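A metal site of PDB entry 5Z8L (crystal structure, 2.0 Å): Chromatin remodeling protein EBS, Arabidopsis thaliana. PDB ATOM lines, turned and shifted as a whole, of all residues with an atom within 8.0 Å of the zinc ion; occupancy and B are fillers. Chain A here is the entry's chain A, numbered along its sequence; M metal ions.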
ATOM      1  N   GLN A  83      20.238 -22.477 -15.055  1.00  0.00           N
ATOM      2  CA  GLN A  83      20.267 -21.354 -14.129  1.00  0.00           C
ATOM      3  C   GLN A  83      21.680 -20.866 -13.810  1.00  0.00           C
ATOM      4  O   GLN A  83      21.877 -19.708 -13.470  1.00  0.00           O
ATOM      5  CB  GLN A  83      19.555 -21.714 -12.823  1.00  0.00           C
ATOM      6  CG  GLN A  83      20.201 -22.855 -12.056  1.00  0.00           C
ATOM      7  CD  GLN A  83      19.822 -22.870 -10.592  1.00  0.00           C
ATOM      8  OE1 GLN A  83      20.651 -22.597  -9.719  1.00  0.00           O
ATOM      9  NE2 GLN A  83      18.566 -23.179 -10.309  1.00  0.00           N
ATOM     10  N   TYR A 148      28.521 -25.105  -5.417  1.00  0.00           N
ATOM     11  CA  TYR A 148      28.527 -24.285  -4.222  1.00  0.00           C
ATOM     12  C   TYR A 148      27.154 -24.097  -3.612  1.00  0.00           C
ATOM     13  O   TYR A 148      26.171 -24.312  -4.250  1.00  0.00           O
ATOM     14  CB  TYR A 148      29.108 -22.944  -4.551  1.00  0.00           C
ATOM     15  CG  TYR A 148      30.462 -22.978  -5.138  1.00  0.00           C
ATOM     16  CD1 TYR A 148      31.555 -22.963  -4.356  1.00  0.00           C
ATOM     17  CD2 TYR A 148      30.639 -23.032  -6.488  1.00  0.00           C
ATOM     18  CE1 TYR A 148      32.809 -22.994  -4.884  1.00  0.00           C
ATOM     19  CE2 TYR A 148      31.891 -23.074  -7.024  1.00  0.00           C
ATOM     20  CZ  TYR A 148      32.967 -23.052  -6.202  1.00  0.00           C
ATOM     21  OH  TYR A 148      34.235 -23.074  -6.661  1.00  0.00           O
ATOM     22  N   CYS A 149      27.108 -23.716  -2.354  1.00  0.00           N
ATOM     23  CA  CYS A 149      25.901 -23.269  -1.690  1.00  0.00           C
ATOM     24  C   CYS A 149      25.008 -24.425  -1.308  1.00  0.00           C
ATOM     25  O   CYS A 149      25.301 -25.541  -1.585  1.00  0.00           O
ATOM     26  CB  CYS A 149      25.111 -22.299  -2.572  1.00  0.00           C
ATOM     27  SG  CYS A 149      23.762 -21.397  -1.806  1.00  0.00           S
ATOM     28  N   LYS A 150      23.890 -24.123  -0.703  1.00  0.00           N
ATOM     29  CA  LYS A 150      22.883 -25.112  -0.395  1.00  0.00           C
ATOM     30  C   LYS A 150      22.328 -25.735  -1.654  1.00  0.00           C
ATOM     31  O   LYS A 150      21.999 -26.866  -1.686  1.00  0.00           O
ATOM     32  CB  LYS A 150      21.739 -24.498   0.403  1.00  0.00           C
ATOM     33  CG  LYS A 150      22.090 -24.191   1.834  1.00  0.00           C
ATOM     34  CD  LYS A 150      20.840 -23.909   2.643  1.00  0.00           C
ATOM     35  CE  LYS A 150      21.171 -23.116   3.878  1.00  0.00           C
ATOM     36  NZ  LYS A 150      19.972 -22.788   4.700  1.00  0.00           N
ATOM     37  N   CYS A 151      22.177 -24.951  -2.692  1.00  0.00           N
ATOM     38  CA  CYS A 151      21.565 -25.389  -3.939  1.00  0.00           C
ATOM     39  C   CYS A 151      22.501 -26.241  -4.798  1.00  0.00           C
ATOM     40  O   CYS A 151      22.126 -26.676  -5.875  1.00  0.00           O
ATOM     41  CB  CYS A 151      21.101 -24.180  -4.745  1.00  0.00           C
ATOM     42  SG  CYS A 151      22.434 -23.056  -5.194  1.00  0.00           S
ATOM     43  N   GLU A 152      23.724 -26.458  -4.298  1.00  0.00           N
ATOM     44  CA  GLU A 152      24.765 -27.277  -4.945  1.00  0.00           C
ATOM     45  C   GLU A 152      24.943 -27.008  -6.443  1.00  0.00           C
ATOM     46  O   GLU A 152      25.125 -27.930  -7.246  1.00  0.00           O
ATOM     47  CB  GLU A 152      24.502 -28.773  -4.689  1.00  0.00           C
ATOM     48  CG  GLU A 152      23.379 -29.447  -5.485  1.00  0.00           C
ATOM     49  CD  GLU A 152      22.063 -29.488  -4.744  1.00  0.00           C
ATOM     50  OE1 GLU A 152      21.976 -28.922  -3.632  1.00  0.00           O
ATOM     51  OE2 GLU A 152      21.102 -30.085  -5.278  1.00  0.00           O
ATOM     52  N   MET A 153      24.918 -25.732  -6.831  1.00  0.00           N
ATOM     53  CA  MET A 153      25.017 -25.354  -8.234  1.00  0.00           C
ATOM     54  C   MET A 153      26.402 -24.801  -8.581  1.00  0.00           C
ATOM     55  O   MET A 153      27.111 -24.296  -7.714  1.00  0.00           O
ATOM     56  CB  MET A 153      23.947 -24.312  -8.559  1.00  0.00           C
ATOM     57  CG  MET A 153      22.535 -24.851  -8.513  1.00  0.00           C
ATOM     58  SD  MET A 153      22.178 -25.922  -9.905  1.00  0.00           S
ATOM     59  CE  MET A 153      20.503 -26.431  -9.532  1.00  0.00           C
ATOM     60  N   PRO A 154      26.780 -24.901  -9.867  1.00  0.00           N
ATOM     61  CA  PRO A 154      27.993 -24.236 -10.347  1.00  0.00           C
ATOM     62  C   PRO A 154      27.903 -22.725 -10.194  1.00  0.00           C
ATOM     63  O   PRO A 154      26.799 -22.180 -10.131  1.00  0.00           O
ATOM     64  CB  PRO A 154      28.057 -24.630 -11.826  1.00  0.00           C
ATOM     65  CG  PRO A 154      27.270 -25.905 -11.910  1.00  0.00           C
ATOM     66  CD  PRO A 154      26.170 -25.747 -10.900  1.00  0.00           C
ATOM     67  N   ASP A 159      25.431 -13.798 -10.323  1.00  0.00           N
ATOM     68  CA  ASP A 159      24.774 -13.832  -9.024  1.00  0.00           C
ATOM     69  C   ASP A 159      25.734 -13.527  -7.884  1.00  0.00           C
ATOM     70  O   ASP A 159      26.802 -14.125  -7.785  1.00  0.00           O
ATOM     71  CB  ASP A 159      24.139 -15.209  -8.782  1.00  0.00           C
ATOM     72  CG  ASP A 159      23.079 -15.543  -9.807  1.00  0.00           C
ATOM     73  OD1 ASP A 159      22.403 -14.608 -10.293  1.00  0.00           O
ATOM     74  OD2 ASP A 159      22.926 -16.737 -10.141  1.00  0.00           O
ATOM     75  N   LEU A 160      25.355 -12.581  -7.031  1.00  0.00           N
ATOM     76  CA  LEU A 160      26.157 -12.259  -5.864  1.00  0.00           C
ATOM     77  C   LEU A 160      26.231 -13.473  -4.948  1.00  0.00           C
ATOM     78  O   LEU A 160      25.245 -14.175  -4.743  1.00  0.00           O
ATOM     79  CB  LEU A 160      25.581 -11.054  -5.123  1.00  0.00           C
ATOM     80  CG  LEU A 160      26.418 -10.381  -4.015  1.00  0.00           C
ATOM     81  CD1 LEU A 160      25.977  -8.943  -3.836  1.00  0.00           C
ATOM     82  CD2 LEU A 160      26.306 -11.121  -2.693  1.00  0.00           C
ATOM     83  N   MET A 161      27.425 -13.730  -4.413  1.00  0.00           N
ATOM     84  CA  MET A 161      27.613 -14.786  -3.433  1.00  0.00           C
ATOM     85  C   MET A 161      28.534 -14.302  -2.323  1.00  0.00           C
ATOM     86  O   MET A 161      29.410 -13.465  -2.560  1.00  0.00           O
ATOM     87  CB  MET A 161      28.186 -16.049  -4.070  1.00  0.00           C
ATOM     88  CG  MET A 161      27.316 -16.657  -5.166  1.00  0.00           C
ATOM     89  SD  MET A 161      27.961 -18.236  -5.749  1.00  0.00           S
ATOM     90  CE  MET A 161      27.358 -19.344  -4.481  1.00  0.00           C
ATOM     91  N   TRP A 170      30.789 -20.861  -0.828  1.00  0.00           N
ATOM     92  CA  TRP A 170      30.095 -19.632  -1.193  1.00  0.00           C
ATOM     93  C   TRP A 170      28.598 -19.845  -1.188  1.00  0.00           C
ATOM     94  O   TRP A 170      28.112 -20.930  -1.494  1.00  0.00           O
ATOM     95  CB  TRP A 170      30.572 -19.152  -2.571  1.00  0.00           C
ATOM     96  CG  TRP A 170      32.014 -18.753  -2.579  1.00  0.00           C
ATOM     97  CD1 TRP A 170      33.105 -19.579  -2.631  1.00  0.00           C
ATOM     98  CD2 TRP A 170      32.537 -17.417  -2.522  1.00  0.00           C
ATOM     99  NE1 TRP A 170      34.260 -18.844  -2.612  1.00  0.00           N
ATOM    100  CE2 TRP A 170      33.945 -17.514  -2.547  1.00  0.00           C
ATOM    101  CE3 TRP A 170      31.952 -16.150  -2.458  1.00  0.00           C
ATOM    102  CZ2 TRP A 170      34.772 -16.395  -2.511  1.00  0.00           C
ATOM    103  CZ3 TRP A 170      32.776 -15.044  -2.416  1.00  0.00           C
ATOM    104  CH2 TRP A 170      34.170 -15.171  -2.447  1.00  0.00           C
ATOM    105  N   TYR A 171      27.847 -18.797  -0.849  1.00  0.00           N
ATOM    106  CA  TYR A 171      26.410 -18.920  -0.702  1.00  0.00           C
ATOM    107  C   TYR A 171      25.655 -17.800  -1.399  1.00  0.00           C
ATOM    108  O   TYR A 171      26.034 -16.632  -1.318  1.00  0.00           O
ATOM    109  CB  TYR A 171      26.022 -18.931   0.782  1.00  0.00           C
ATOM    110  CG  TYR A 171      26.447 -20.169   1.527  1.00  0.00           C
ATOM    111  CD1 TYR A 171      27.684 -20.223   2.151  1.00  0.00           C
ATOM    112  CD2 TYR A 171      25.614 -21.273   1.614  1.00  0.00           C
ATOM    113  CE1 TYR A 171      28.085 -21.356   2.842  1.00  0.00           C
ATOM    114  CE2 TYR A 171      26.004 -22.406   2.296  1.00  0.00           C
ATOM    115  CZ  TYR A 171      27.234 -22.448   2.905  1.00  0.00           C
ATOM    116  OH  TYR A 171      27.619 -23.577   3.593  1.00  0.00           O
ATOM    117  N   HIS A 172      24.576 -18.168  -2.091  1.00  0.00           N
ATOM    118  CA  HIS A 172      23.591 -17.192  -2.519  1.00  0.00           C
ATOM    119  C   HIS A 172      22.861 -16.696  -1.265  1.00  0.00           C
ATOM    120  O   HIS A 172      22.410 -17.493  -0.463  1.00  0.00           O
ATOM    121  CB  HIS A 172      22.579 -17.797  -3.498  1.00  0.00           C
ATOM    122  CG  HIS A 172      23.199 -18.376  -4.730  1.00  0.00           C
ATOM    123  ND1 HIS A 172      23.410 -19.729  -4.889  1.00  0.00           N
ATOM    124  CD2 HIS A 172      23.666 -17.791  -5.856  1.00  0.00           C
ATOM    125  CE1 HIS A 172      23.973 -19.950  -6.067  1.00  0.00           C
ATOM    126  NE2 HIS A 172      24.133 -18.788  -6.667  1.00  0.00           N
ATOM    127  N   PRO A 173      22.776 -15.366  -1.097  1.00  0.00           N
ATOM    128  CA  PRO A 173      22.055 -14.780   0.036  1.00  0.00           C
ATOM    129  C   PRO A 173      20.633 -15.337   0.180  1.00  0.00           C
ATOM    130  O   PRO A 173      20.246 -15.727   1.280  1.00  0.00           O
ATOM    131  CB  PRO A 173      22.024 -13.292  -0.315  1.00  0.00           C
ATOM    132  CG  PRO A 173      23.275 -13.087  -1.099  1.00  0.00           C
ATOM    133  CD  PRO A 173      23.458 -14.346  -1.915  1.00  0.00           C
ATOM    134  N   ALA A 174      19.888 -15.390  -0.919  1.00  0.00           N
ATOM    135  CA  ALA A 174      18.512 -15.890  -0.884  1.00  0.00           C
ATOM    136  C   ALA A 174      18.441 -17.318  -0.346  1.00  0.00           C
ATOM    137  O   ALA A 174      17.477 -17.690   0.315  1.00  0.00           O
ATOM    138  CB  ALA A 174      17.882 -15.815  -2.268  1.00  0.00           C
ATOM    139  N   CYS A 175      19.472 -18.113  -0.632  1.00  0.00           N
ATOM    140  CA  CYS A 175      19.517 -19.496  -0.176  1.00  0.00           C
ATOM    141  C   CYS A 175      19.774 -19.609   1.312  1.00  0.00           C
ATOM    142  O   CYS A 175      19.438 -20.622   1.932  1.00  0.00           O
ATOM    143  CB  CYS A 175      20.579 -20.271  -0.945  1.00  0.00           C
ATOM    144  SG  CYS A 175      20.245 -20.452  -2.703  1.00  0.00           S
ATOM    145  N   VAL A 176      20.387 -18.586   1.905  1.00  0.00           N
ATOM    146  CA  VAL A 176      20.630 -18.605   3.340  1.00  0.00           C
ATOM    147  C   VAL A 176      19.697 -17.633   4.049  1.00  0.00           C
ATOM    148  O   VAL A 176      19.938 -17.233   5.185  1.00  0.00           O
ATOM    149  CB  VAL A 176      22.107 -18.274   3.681  1.00  0.00           C
ATOM    150  CG1 VAL A 176      23.017 -19.410   3.243  1.00  0.00           C
ATOM    151  CG2 VAL A 176      22.531 -16.965   3.030  1.00  0.00           C
HETATM  152 ZN    ZN M   1      22.286 -21.173  -3.664  1.00  0.00          ZN
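The backbone carbonyl oxygen of Trp 170 sits at hydrogen-bond distance from the backbone NH of Cys 149 (3.1 Å).
Within 4 Å of the zinc ion: Cys 149, Cys 151, His 172 and Cys 175.
The nearest printed residue that does not touch the zinc ion is Lys 150 (4.5 Å).
The zinc ion is bound by ND1 of His 172 (2.2 Å), SG of Cys 175 (2.4 Å), SG of Cys 149 (2.4 Å) and SG of Cys 151 (2.4 Å).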
